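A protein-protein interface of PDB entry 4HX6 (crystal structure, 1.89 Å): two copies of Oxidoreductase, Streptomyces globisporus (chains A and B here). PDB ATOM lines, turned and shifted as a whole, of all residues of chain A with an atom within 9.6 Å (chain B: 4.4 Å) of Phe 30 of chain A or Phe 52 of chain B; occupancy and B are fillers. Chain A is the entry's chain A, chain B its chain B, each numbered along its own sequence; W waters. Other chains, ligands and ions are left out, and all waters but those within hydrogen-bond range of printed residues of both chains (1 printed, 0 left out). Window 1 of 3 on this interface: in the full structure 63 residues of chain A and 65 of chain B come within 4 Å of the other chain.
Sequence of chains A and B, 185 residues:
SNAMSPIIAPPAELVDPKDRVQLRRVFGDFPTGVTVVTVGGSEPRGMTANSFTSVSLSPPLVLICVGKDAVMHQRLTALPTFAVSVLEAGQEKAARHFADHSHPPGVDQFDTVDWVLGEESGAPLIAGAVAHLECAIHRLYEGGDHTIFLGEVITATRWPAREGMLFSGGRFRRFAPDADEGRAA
Among the printed residues, pairs that only touch across the chains: Phe 30 of chain A with Phe 52 of chain B (3.4 Å), Phe 30 of chain A with Gly 33 of chain B (3.4 Å), Pro 31 of chain A with Thr 32 of chain B (3.5 Å), Thr 53 of chain A with Ser 51 of chain B (3.6 Å), Phe 30 of chain A with Thr 35 of chain B (3.6 Å), Phe 30 of chain A with Val 34 of chain B (3.6 Å), Phe 27 of chain A with Val 62 of chain B (3.6 Å), Thr 53 of chain A with Thr 53 of chain B (3.7 Å), Ser 51 of chain A with Thr 53 of chain B (3.7 Å), Asp 29 of chain A with Val 86 of chain B (3.9 Å), Phe 30 of chain A with Asn 50 of chain B (3.9 Å) and Leu 63 of chain A with Leu 63 of chain B (3.9 Å).
Water W1 lies within hydrogen-bond range of the backbone carbonyl oxygen (O) of Asn 50 of chain A (2.6 Å), the backbone carbonyl oxygen (O) of Phe 52 of chain A (3.1 Å) and the side-chain hydroxyl (OG1) of Thr 53 of chain B (3.4 Å).
O of Pro 31 of chain A sits at hydrogen-bond distance from N of Gly 33 of chain B, at 2.9 Å.
Phe 52 of chain B touches one residue of chain A.
Gly 33 of chain B touches just these residues of chain A: Phe 30 (3.4 Å) and Pro 31 (2.9 Å).
Of chain A, only Thr 53 (3.6 Å) comes within 4 Å of Ser 51 of chain B.
Of the printed residues of chain B, Phe 27 of chain A touches Val 62.
Of the printed residues of chain A, Leu 63 of chain B touches Leu 63 (3.9 Å).
Arg 24 of chain A touches none of the printed residues of chain B.
Ser 54 of chain A touches none of the printed residues of chain B.
The nearest residue of chain A that does not touch Phe 52 of chain B is Thr 53 of chain A (4.8 Å).
The nearest printed residue of chain A that does not touch Thr 32 of chain B is Phe 30 of chain A (4.2 Å).
Along chain B the printed residues that touch a printed residue of chain A span positions 32 to 86.
Ser 51 of chain A touches Thr 53 of chain B, and with the chains exchanged Thr 53 of chain A touches Ser 51 of chain B.
Thr 53 of chain B touches its own counterpart, Thr 53 of chain A.
Leu 63 of chain A touches its own counterpart, Leu 63 of chain B.
Positions printed for both chains: 32, 33, 50, 51, 52, 53 and 63.
Of the 13 pairs that touch across the chains among the printed residues, 4 have their exchanged pair printed and touching as well.
ND2 of Asn 50 of chain B lies within hydrogen-bond range of OG1 of Thr 32 of chain B, 3.2 Å away.
The backbone NH of Leu 63 of chain B sits at hydrogen-bond distance from the backbone carbonyl oxygen of Thr 53 of chain B, 2.9 Å away.
The backbone carbonyl oxygen (O) of Thr 53 of chain A sits at hydrogen-bond distance from the backbone NH (N) of Leu 63 of chain A, 2.8 Å away.
The side-chain hydroxyl of Thr 53 of chain A lies within hydrogen-bond range of the backbone carbonyl oxygen of Ser 51 of chain A.
OG of Ser 51 of chain A sits at hydrogen-bond distance from N of Cys 65 of chain A, at 2.8 Å.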
ATOM      1  N   LEU A  23     -31.608 -21.359  -7.461  1.00  0.00           N
ATOM      2  CA  LEU A  23     -30.343 -22.043  -7.669  1.00  0.00           C
ATOM      3  C   LEU A  23     -29.567 -22.143  -6.367  1.00  0.00           C
ATOM      4  O   LEU A  23     -28.961 -23.187  -6.073  1.00  0.00           O
ATOM      5  CB  LEU A  23     -29.510 -21.330  -8.740  1.00  0.00           C
ATOM      6  CG  LEU A  23     -28.226 -22.042  -9.158  1.00  0.00           C
ATOM      7  CD1 LEU A  23     -28.546 -23.380  -9.814  1.00  0.00           C
ATOM      8  CD2 LEU A  23     -27.409 -21.144 -10.093  1.00  0.00           C
ATOM      9  N   ARG A  24     -29.578 -21.072  -5.571  1.00  0.00           N
ATOM     10  CA  ARG A  24     -28.908 -21.117  -4.269  1.00  0.00           C
ATOM     11  C   ARG A  24     -29.484 -22.244  -3.428  1.00  0.00           C
ATOM     12  O   ARG A  24     -28.760 -22.924  -2.687  1.00  0.00           O
ATOM     13  CB  ARG A  24     -29.086 -19.809  -3.488  1.00  0.00           C
ATOM     14  CG  ARG A  24     -28.194 -18.663  -3.929  1.00  0.00           C
ATOM     15  CD  ARG A  24     -28.302 -17.505  -2.937  1.00  0.00           C
ATOM     16  NE  ARG A  24     -28.046 -16.209  -3.564  1.00  0.00           N
ATOM     17  CZ  ARG A  24     -26.887 -15.556  -3.491  1.00  0.00           C
ATOM     18  NH1 ARG A  24     -26.747 -14.382  -4.095  1.00  0.00           N
ATOM     19  NH2 ARG A  24     -25.869 -16.078  -2.816  1.00  0.00           N
ATOM     20  N   ARG A  25     -30.796 -22.421  -3.516  1.00  0.00           N
ATOM     21  CA  ARG A  25     -31.454 -23.461  -2.749  1.00  0.00           C
ATOM     22  C   ARG A  25     -31.009 -24.866  -3.153  1.00  0.00           C
ATOM     23  O   ARG A  25     -30.804 -25.707  -2.286  1.00  0.00           O
ATOM     24  CB  ARG A  25     -32.977 -23.310  -2.772  1.00  0.00           C
ATOM     25  CG  ARG A  25     -33.485 -22.412  -1.642  1.00  0.00           C
ATOM     26  CD  ARG A  25     -34.669 -21.565  -2.043  1.00  0.00           C
ATOM     27  NE  ARG A  25     -35.738 -22.339  -2.662  1.00  0.00           N
ATOM     28  CZ  ARG A  25     -36.811 -21.791  -3.221  1.00  0.00           C
ATOM     29  NH1 ARG A  25     -36.951 -20.472  -3.228  1.00  0.00           N
ATOM     30  NH2 ARG A  25     -37.744 -22.556  -3.770  1.00  0.00           N
ATOM     31  N   VAL A  26     -30.839 -25.147  -4.443  1.00  0.00           N
ATOM     32  CA  VAL A  26     -30.379 -26.485  -4.802  1.00  0.00           C
ATOM     33  C   VAL A  26     -28.907 -26.665  -4.428  1.00  0.00           C
ATOM     34  O   VAL A  26     -28.507 -27.734  -3.986  1.00  0.00           O
ATOM     35  CB  VAL A  26     -30.654 -26.863  -6.282  1.00  0.00           C
ATOM     36  CG1 VAL A  26     -29.901 -25.946  -7.223  1.00  0.00           C
ATOM     37  CG2 VAL A  26     -30.275 -28.326  -6.534  1.00  0.00           C
ATOM     38  N   PHE A  27     -28.105 -25.618  -4.582  1.00  0.00           N
ATOM     39  CA  PHE A  27     -26.698 -25.716  -4.190  1.00  0.00           C
ATOM     40  C   PHE A  27     -26.621 -26.021  -2.688  1.00  0.00           C
ATOM     41  O   PHE A  27     -25.759 -26.776  -2.229  1.00  0.00           O
ATOM     42  CB  PHE A  27     -25.932 -24.431  -4.513  1.00  0.00           C
ATOM     43  CG  PHE A  27     -25.595 -24.248  -5.991  1.00  0.00           C
ATOM     44  CD1 PHE A  27     -25.841 -25.253  -6.917  1.00  0.00           C
ATOM     45  CD2 PHE A  27     -25.006 -23.072  -6.430  1.00  0.00           C
ATOM     46  CE1 PHE A  27     -25.528 -25.083  -8.267  1.00  0.00           C
ATOM     47  CE2 PHE A  27     -24.672 -22.893  -7.771  1.00  0.00           C
ATOM     48  CZ  PHE A  27     -24.940 -23.899  -8.693  1.00  0.00           C
ATOM     49  N   GLY A  28     -27.536 -25.436  -1.933  1.00  0.00           N
ATOM     50  CA  GLY A  28     -27.580 -25.620  -0.491  1.00  0.00           C
ATOM     51  C   GLY A  28     -28.002 -27.017  -0.072  1.00  0.00           C
ATOM     52  O   GLY A  28     -27.890 -27.371   1.096  1.00  0.00           O
ATOM     53  N   ASP A  29     -28.478 -27.819  -1.024  1.00  0.00           N
ATOM     54  CA  ASP A  29     -28.990 -29.148  -0.713  1.00  0.00           C
ATOM     55  C   ASP A  29     -27.873 -30.170  -0.491  1.00  0.00           C
ATOM     56  O   ASP A  29     -28.118 -31.265   0.006  1.00  0.00           O
ATOM     57  CB  ASP A  29     -29.926 -29.639  -1.819  1.00  0.00           C
ATOM     58  CG  ASP A  29     -31.301 -29.004  -1.743  1.00  0.00           C
ATOM     59  OD1 ASP A  29     -31.665 -28.494  -0.663  1.00  0.00           O
ATOM     60  OD2 ASP A  29     -32.028 -29.024  -2.761  1.00  0.00           O
ATOM     61  N   PHE A  30     -26.653 -29.810  -0.872  1.00  0.00           N
ATOM     62  CA  PHE A  30     -25.500 -30.678  -0.693  1.00  0.00           C
ATOM     63  C   PHE A  30     -24.805 -30.269   0.603  1.00  0.00           C
ATOM     64  O   PHE A  30     -24.267 -29.163   0.690  1.00  0.00           O
ATOM     65  CB  PHE A  30     -24.526 -30.542  -1.884  1.00  0.00           C
ATOM     66  CG  PHE A  30     -23.341 -31.470  -1.804  1.00  0.00           C
ATOM     67  CD1 PHE A  30     -23.458 -32.796  -2.174  1.00  0.00           C
ATOM     68  CD2 PHE A  30     -22.111 -31.013  -1.347  1.00  0.00           C
ATOM     69  CE1 PHE A  30     -22.373 -33.661  -2.091  1.00  0.00           C
ATOM     70  CE2 PHE A  30     -21.014 -31.874  -1.266  1.00  0.00           C
ATOM     71  CZ  PHE A  30     -21.148 -33.196  -1.634  1.00  0.00           C
ATOM     72  N   PRO A  31     -24.826 -31.149   1.617  1.00  0.00           N
ATOM     73  CA  PRO A  31     -24.252 -30.808   2.926  1.00  0.00           C
ATOM     74  C   PRO A  31     -22.736 -30.684   2.860  1.00  0.00           C
ATOM     75  O   PRO A  31     -22.100 -31.355   2.044  1.00  0.00           O
ATOM     76  CB  PRO A  31     -24.637 -32.005   3.809  1.00  0.00           C
ATOM     77  CG  PRO A  31     -25.668 -32.766   3.051  1.00  0.00           C
ATOM     78  CD  PRO A  31     -25.406 -32.501   1.605  1.00  0.00           C
ATOM     79  N   THR A  32     -22.166 -29.825   3.700  1.00  0.00           N
ATOM     80  CA  THR A  32     -20.722 -29.672   3.761  1.00  0.00           C
ATOM     81  C   THR A  32     -20.246 -29.348   5.170  1.00  0.00           C
ATOM     82  O   THR A  32     -21.040 -29.056   6.067  1.00  0.00           O
ATOM     83  CB  THR A  32     -20.204 -28.520   2.843  1.00  0.00           C
ATOM     84  OG1 THR A  32     -20.686 -27.261   3.323  1.00  0.00           O
ATOM     85  CG2 THR A  32     -20.629 -28.718   1.382  1.00  0.00           C
ATOM     86  N   GLY A  33     -18.932 -29.378   5.355  1.00  0.00           N
ATOM     87  CA  GLY A  33     -18.349 -28.807   6.550  1.00  0.00           C
ATOM     88  C   GLY A  33     -18.251 -27.296   6.401  1.00  0.00           C
ATOM     89  O   GLY A  33     -18.785 -26.713   5.454  1.00  0.00           O
ATOM     90  N   ASN A  50     -17.407 -22.821   2.417  1.00  0.00           N
ATOM     91  CA  ASN A  50     -17.826 -24.216   2.424  1.00  0.00           C
ATOM     92  C   ASN A  50     -17.491 -24.908   1.107  1.00  0.00           C
ATOM     93  O   ASN A  50     -17.861 -26.062   0.893  1.00  0.00           O
ATOM     94  CB  ASN A  50     -19.320 -24.322   2.706  1.00  0.00           C
ATOM     95  CG  ASN A  50     -20.143 -23.478   1.760  1.00  0.00           C
ATOM     96  OD1 ASN A  50     -19.711 -23.178   0.650  1.00  0.00           O
ATOM     97  ND2 ASN A  50     -21.330 -23.074   2.203  1.00  0.00           N
ATOM     98  N   SER A  51     -16.779 -24.198   0.226  1.00  0.00           N
ATOM     99  CA  SER A  51     -16.453 -24.737  -1.092  1.00  0.00           C
ATOM    100  C   SER A  51     -15.178 -25.570  -1.104  1.00  0.00           C
ATOM    101  O   SER A  51     -14.746 -26.050  -2.152  1.00  0.00           O
ATOM    102  CB  SER A  51     -16.331 -23.610  -2.119  1.00  0.00           C
ATOM    103  OG  SER A  51     -15.113 -22.919  -1.931  1.00  0.00           O
ATOM    104  N   PHE A  52     -14.581 -25.749   0.063  1.00  0.00           N
ATOM    105  CA  PHE A  52     -13.367 -26.530   0.173  1.00  0.00           C
ATOM    106  C   PHE A  52     -13.549 -27.962  -0.349  1.00  0.00           C
ATOM    107  O   PHE A  52     -14.495 -28.640   0.021  1.00  0.00           O
ATOM    108  CB  PHE A  52     -12.930 -26.554   1.635  1.00  0.00           C
ATOM    109  CG  PHE A  52     -11.769 -27.450   1.896  1.00  0.00           C
ATOM    110  CD1 PHE A  52     -10.480 -27.032   1.617  1.00  0.00           C
ATOM    111  CD2 PHE A  52     -11.963 -28.720   2.405  1.00  0.00           C
ATOM    112  CE1 PHE A  52      -9.396 -27.869   1.868  1.00  0.00           C
ATOM    113  CE2 PHE A  52     -10.895 -29.558   2.650  1.00  0.00           C
ATOM    114  CZ  PHE A  52      -9.609 -29.134   2.382  1.00  0.00           C
ATOM    115  N   THR A  53     -12.637 -28.442  -1.184  1.00  0.00           N
ATOM    116  CA  THR A  53     -12.777 -29.798  -1.716  1.00  0.00           C
ATOM    117  C   THR A  53     -11.401 -30.455  -1.793  1.00  0.00           C
ATOM    118  O   THR A  53     -10.467 -29.838  -2.303  1.00  0.00           O
ATOM    119  CB  THR A  53     -13.371 -29.760  -3.141  1.00  0.00           C
ATOM    120  OG1 THR A  53     -14.605 -29.030  -3.130  1.00  0.00           O
ATOM    121  CG2 THR A  53     -13.612 -31.168  -3.673  1.00  0.00           C
ATOM    122  N   SER A  54     -11.250 -31.685  -1.303  1.00  0.00           N
ATOM    123  CA  SER A  54      -9.969 -32.373  -1.530  1.00  0.00           C
ATOM    124  C   SER A  54      -9.929 -32.883  -2.980  1.00  0.00           C
ATOM    125  O   SER A  54     -10.923 -33.404  -3.495  1.00  0.00           O
ATOM    126  CB  SER A  54      -9.753 -33.513  -0.543  1.00  0.00           C
ATOM    127  OG  SER A  54     -10.804 -34.454  -0.642  1.00  0.00           O
ATOM    128  N   VAL A  55      -8.788 -32.721  -3.641  1.00  0.00           N
ATOM    129  CA  VAL A  55      -8.710 -33.028  -5.061  1.00  0.00           C
ATOM    130  C   VAL A  55      -7.853 -34.257  -5.379  1.00  0.00           C
ATOM    131  O   VAL A  55      -8.274 -35.133  -6.140  1.00  0.00           O
ATOM    132  CB  VAL A  55      -8.182 -31.825  -5.858  1.00  0.00           C
ATOM    133  CG1 VAL A  55      -8.085 -32.181  -7.333  1.00  0.00           C
ATOM    134  CG2 VAL A  55      -9.102 -30.589  -5.622  1.00  0.00           C
ATOM    135  N   LEU A  63      -8.892 -27.786  -3.429  1.00  0.00           N
ATOM    136  CA  LEU A  63      -9.340 -26.532  -4.042  1.00  0.00           C
ATOM    137  C   LEU A  63     -10.312 -25.751  -3.174  1.00  0.00           C
ATOM    138  O   LEU A  63     -10.998 -26.309  -2.294  1.00  0.00           O
ATOM    139  CB  LEU A  63      -9.898 -26.738  -5.470  1.00  0.00           C
ATOM    140  CG  LEU A  63     -11.194 -27.557  -5.653  1.00  0.00           C
ATOM    141  CD1 LEU A  63     -12.427 -26.709  -5.323  1.00  0.00           C
ATOM    142  CD2 LEU A  63     -11.311 -28.072  -7.087  1.00  0.00           C
ATOM    143  N   CYS A  65     -13.202 -22.279  -3.813  1.00  0.00           N
ATOM    144  CA  CYS A  65     -13.771 -21.368  -4.801  1.00  0.00           C
ATOM    145  C   CYS A  65     -14.018 -20.054  -4.079  1.00  0.00           C
ATOM    146  O   CYS A  65     -14.635 -20.034  -3.026  1.00  0.00           O
ATOM    147  CB  CYS A  65     -15.077 -21.914  -5.394  1.00  0.00           C
ATOM    148  SG  CYS A  65     -14.936 -23.544  -6.205  1.00  0.00           S
ATOM    149  N   LEU A 166     -21.187 -28.696  10.641  1.00  0.00           N
ATOM    150  CA  LEU A 166     -21.934 -29.049   9.431  1.00  0.00           C
ATOM    151  C   LEU A 166     -22.722 -27.843   8.955  1.00  0.00           C
ATOM    152  O   LEU A 166     -23.133 -27.018   9.760  1.00  0.00           O
ATOM    153  CB  LEU A 166     -22.916 -30.177   9.731  1.00  0.00           C
ATOM    154  CG  LEU A 166     -22.337 -31.579   9.844  1.00  0.00           C
ATOM    155  CD1 LEU A 166     -23.452 -32.584  10.147  1.00  0.00           C
ATOM    156  CD2 LEU A 166     -21.627 -31.946   8.553  1.00  0.00           C
ATOM    157  N   PHE A 167     -22.941 -27.744   7.648  1.00  0.00           N
ATOM    158  CA  PHE A 167     -23.738 -26.660   7.095  1.00  0.00           C
ATOM    159  C   PHE A 167     -24.597 -27.226   5.995  1.00  0.00           C
ATOM    160  O   PHE A 167     -24.105 -27.942   5.128  1.00  0.00           O
ATOM    161  CB  PHE A 167     -22.841 -25.578   6.504  1.00  0.00           C
ATOM    162  CG  PHE A 167     -23.528 -24.257   6.336  1.00  0.00           C
ATOM    163  CD1 PHE A 167     -23.752 -23.441   7.433  1.00  0.00           C
ATOM    164  CD2 PHE A 167     -23.941 -23.825   5.085  1.00  0.00           C
ATOM    165  CE1 PHE A 167     -24.383 -22.223   7.287  1.00  0.00           C
ATOM    166  CE2 PHE A 167     -24.570 -22.609   4.931  1.00  0.00           C
ATOM    167  CZ  PHE A 167     -24.792 -21.808   6.033  1.00  0.00           C
ATOM    168  N   SER A 168     -25.883 -26.919   6.026  1.00  0.00           N
ATOM    169  CA  SER A 168     -26.785 -27.446   5.014  1.00  0.00           C
ATOM    170  C   SER A 168     -28.069 -26.627   4.987  1.00  0.00           C
ATOM    171  O   SER A 168     -28.541 -26.166   6.030  1.00  0.00           O
ATOM    172  CB  SER A 168     -27.085 -28.918   5.302  1.00  0.00           C
ATOM    173  OG  SER A 168     -27.789 -29.515   4.228  1.00  0.00           O
ATOM    174  N   GLY A 169     -28.636 -26.442   3.797  1.00  0.00           N
ATOM    175  CA  GLY A 169     -29.857 -25.662   3.673  1.00  0.00           C
ATOM    176  C   GLY A 169     -29.677 -24.305   4.327  1.00  0.00           C
ATOM    177  O   GLY A 169     -30.583 -23.799   4.987  1.00  0.00           O
ATOM    178  N   GLY A 170     -28.488 -23.729   4.163  1.00  0.00           N
ATOM    179  CA  GLY A 170     -28.170 -22.431   4.738  1.00  0.00           C
ATOM    180  C   GLY A 170     -28.192 -22.344   6.257  1.00  0.00           C
ATOM    181  O   GLY A 170     -28.342 -21.257   6.814  1.00  0.00           O
ATOM    182  N   ARG A 171     -28.043 -23.472   6.940  1.00  0.00           N
ATOM    183  CA  ARG A 171     -27.992 -23.450   8.405  1.00  0.00           C
ATOM    184  C   ARG A 171     -26.919 -24.363   9.015  1.00  0.00           C
ATOM    185  O   ARG A 171     -26.495 -25.342   8.396  1.00  0.00           O
ATOM    186  CB  ARG A 171     -29.366 -23.770   8.994  1.00  0.00           C
ATOM    187  CG  ARG A 171     -29.950 -25.092   8.540  1.00  0.00           C
ATOM    188  CD  ARG A 171     -31.358 -25.291   9.091  1.00  0.00           C
ATOM    189  NE  ARG A 171     -32.229 -24.159   8.796  1.00  0.00           N
ATOM    190  N   THR B  32     -18.836 -34.107   4.055  1.00  0.00           N
ATOM    191  CA  THR B  32     -19.488 -33.776   2.788  1.00  0.00           C
ATOM    192  C   THR B  32     -20.759 -34.563   2.618  1.00  0.00           C
ATOM    193  O   THR B  32     -21.041 -35.510   3.373  1.00  0.00           O
ATOM    194  CB  THR B  32     -18.626 -34.103   1.535  1.00  0.00           C
ATOM    195  OG1 THR B  32     -18.579 -35.523   1.340  1.00  0.00           O
ATOM    196  CG2 THR B  32     -17.216 -33.550   1.655  1.00  0.00           C
ATOM    197  N   GLY B  33     -21.522 -34.184   1.592  1.00  0.00           N
ATOM    198  CA  GLY B  33     -22.622 -35.000   1.154  1.00  0.00           C
ATOM    199  C   GLY B  33     -22.078 -36.094   0.258  1.00  0.00           C
ATOM    200  O   GLY B  33     -20.862 -36.329   0.188  1.00  0.00           O
ATOM    201  N   VAL B  34     -22.987 -36.765  -0.438  1.00  0.00           N
ATOM    202  CA  VAL B  34     -22.640 -37.861  -1.325  1.00  0.00           C
ATOM    203  C   VAL B  34     -23.525 -37.756  -2.561  1.00  0.00           C
ATOM    204  O   VAL B  34     -24.733 -37.590  -2.446  1.00  0.00           O
ATOM    205  CB  VAL B  34     -22.907 -39.228  -0.658  1.00  0.00           C
ATOM    206  CG1 VAL B  34     -22.455 -40.371  -1.573  1.00  0.00           C
ATOM    207  CG2 VAL B  34     -22.204 -39.313   0.676  1.00  0.00           C
ATOM    208  N   THR B  35     -22.926 -37.862  -3.739  1.00  0.00           N
ATOM    209  CA  THR B  35     -23.700 -37.823  -4.973  1.00  0.00           C
ATOM    210  C   THR B  35     -23.441 -39.064  -5.807  1.00  0.00           C
ATOM    211  O   THR B  35     -22.475 -39.794  -5.584  1.00  0.00           O
ATOM    212  CB  THR B  35     -23.294 -36.638  -5.867  1.00  0.00           C
ATOM    213  OG1 THR B  35     -21.983 -36.876  -6.387  1.00  0.00           O
ATOM    214  CG2 THR B  35     -23.307 -35.330  -5.099  1.00  0.00           C
ATOM    215  N   ASN B  50     -17.964 -37.778  -3.799  1.00  0.00           N
ATOM    216  CA  ASN B  50     -18.230 -36.712  -2.838  1.00  0.00           C
ATOM    217  C   ASN B  50     -17.446 -35.447  -3.108  1.00  0.00           C
ATOM    218  O   ASN B  50     -17.506 -34.519  -2.330  1.00  0.00           O
ATOM    219  CB  ASN B  50     -18.000 -37.174  -1.404  1.00  0.00           C
ATOM    220  CG  ASN B  50     -16.539 -37.417  -1.091  1.00  0.00           C
ATOM    221  OD1 ASN B  50     -15.732 -37.697  -1.980  1.00  0.00           O
ATOM    222  ND2 ASN B  50     -16.192 -37.320   0.187  1.00  0.00           N
ATOM    223  N   SER B  51     -16.721 -35.415  -4.219  1.00  0.00           N
ATOM    224  CA  SER B  51     -15.888 -34.265  -4.562  1.00  0.00           C
ATOM    225  C   SER B  51     -16.675 -33.169  -5.284  1.00  0.00           C
ATOM    226  O   SER B  51     -16.102 -32.300  -5.936  1.00  0.00           O
ATOM    227  CB  SER B  51     -14.741 -34.718  -5.446  1.00  0.00           C
ATOM    228  OG  SER B  51     -15.251 -35.385  -6.597  1.00  0.00           O
ATOM    229  N   PHE B  52     -17.990 -33.213  -5.154  1.00  0.00           N
ATOM    230  CA  PHE B  52     -18.872 -32.262  -5.818  1.00  0.00           C
ATOM    231  C   PHE B  52     -18.934 -30.943  -5.047  1.00  0.00           C
ATOM    232  O   PHE B  52     -19.007 -30.944  -3.816  1.00  0.00           O
ATOM    233  CB  PHE B  52     -20.271 -32.879  -5.944  1.00  0.00           C
ATOM    234  CG  PHE B  52     -21.348 -31.892  -6.297  1.00  0.00           C
ATOM    235  CD1 PHE B  52     -21.678 -31.654  -7.617  1.00  0.00           C
ATOM    236  CD2 PHE B  52     -22.026 -31.198  -5.308  1.00  0.00           C
ATOM    237  CE1 PHE B  52     -22.668 -30.733  -7.949  1.00  0.00           C
ATOM    238  CE2 PHE B  52     -23.015 -30.284  -5.629  1.00  0.00           C
ATOM    239  CZ  PHE B  52     -23.339 -30.048  -6.950  1.00  0.00           C
ATOM    240  N   THR B  53     -18.829 -29.816  -5.747  1.00  0.00           N
ATOM    241  CA  THR B  53     -19.105 -28.526  -5.106  1.00  0.00           C
ATOM    242  C   THR B  53     -19.726 -27.551  -6.079  1.00  0.00           C
ATOM    243  O   THR B  53     -19.534 -27.632  -7.297  1.00  0.00           O
ATOM    244  CB  THR B  53     -17.857 -27.873  -4.441  1.00  0.00           C
ATOM    245  OG1 THR B  53     -18.278 -26.820  -3.559  1.00  0.00           O
ATOM    246  CG2 THR B  53     -16.910 -27.291  -5.486  1.00  0.00           C
ATOM    247  N   VAL B  62     -21.024 -25.941 -11.519  1.00  0.00           N
ATOM    248  CA  VAL B  62     -20.639 -26.874 -10.479  1.00  0.00           C
ATOM    249  C   VAL B  62     -19.400 -27.615 -10.948  1.00  0.00           C
ATOM    250  O   VAL B  62     -19.040 -27.561 -12.125  1.00  0.00           O
ATOM    251  CB  VAL B  62     -21.741 -27.920 -10.195  1.00  0.00           C
ATOM    252  CG1 VAL B  62     -23.018 -27.239  -9.732  1.00  0.00           C
ATOM    253  CG2 VAL B  62     -21.992 -28.789 -11.436  1.00  0.00           C
ATOM    254  N   LEU B  63     -18.741 -28.309 -10.029  1.00  0.00           N
ATOM    255  CA  LEU B  63     -17.606 -29.126 -10.418  1.00  0.00           C
ATOM    256  C   LEU B  63     -17.600 -30.457  -9.698  1.00  0.00           C
ATOM    257  O   LEU B  63     -18.125 -30.585  -8.596  1.00  0.00           O
ATOM    258  CB  LEU B  63     -16.286 -28.383 -10.183  1.00  0.00           C
ATOM    259  CG  LEU B  63     -15.781 -28.076  -8.771  1.00  0.00           C
ATOM    260  CD1 LEU B  63     -15.232 -29.319  -8.074  1.00  0.00           C
ATOM    261  CD2 LEU B  63     -14.675 -27.020  -8.865  1.00  0.00           C
ATOM    262  N   ILE B  64     -17.009 -31.456 -10.344  1.00  0.00           N
ATOM    263  CA  ILE B  64     -16.744 -32.741  -9.696  1.00  0.00           C
ATOM    264  C   ILE B  64     -15.308 -33.131 -10.014  1.00  0.00           C
ATOM    265  O   ILE B  64     -14.783 -32.754 -11.064  1.00  0.00           O
ATOM    266  CB  ILE B  64     -17.700 -33.831 -10.204  1.00  0.00           C
ATOM    267  CG1 ILE B  64     -17.626 -33.918 -11.736  1.00  0.00           C
ATOM    268  CG2 ILE B  64     -19.109 -33.529  -9.758  1.00  0.00           C
ATOM    269  CD1 ILE B  64     -18.493 -34.991 -12.326  1.00  0.00           C
ATOM    270  N   VAL B  84     -25.984 -35.112 -11.921  1.00  0.00           N
ATOM    271  CA  VAL B  84     -25.595 -35.337 -10.542  1.00  0.00           C
ATOM    272  C   VAL B  84     -26.855 -35.556  -9.725  1.00  0.00           C
ATOM    273  O   VAL B  84     -27.793 -34.747  -9.795  1.00  0.00           O
ATOM    274  CB  VAL B  84     -24.837 -34.127  -9.974  1.00  0.00           C
ATOM    275  CG1 VAL B  84     -24.430 -34.378  -8.518  1.00  0.00           C
ATOM    276  CG2 VAL B  84     -23.613 -33.822 -10.838  1.00  0.00           C
ATOM    277  N   VAL B  86     -27.910 -35.858  -5.833  1.00  0.00           N
ATOM    278  CA  VAL B  86     -27.452 -35.694  -4.454  1.00  0.00           C
ATOM    279  C   VAL B  86     -28.218 -36.690  -3.595  1.00  0.00           C
ATOM    280  O   VAL B  86     -29.448 -36.636  -3.537  1.00  0.00           O
ATOM    281  CB  VAL B  86     -27.726 -34.266  -3.963  1.00  0.00           C
ATOM    282  CG1 VAL B  86     -27.397 -34.139  -2.479  1.00  0.00           C
ATOM    283  CG2 VAL B  86     -26.931 -33.259  -4.805  1.00  0.00           C
HETATM  284  O   HOH W   1     -17.530 -28.148  -0.573  1.00  0.00           O
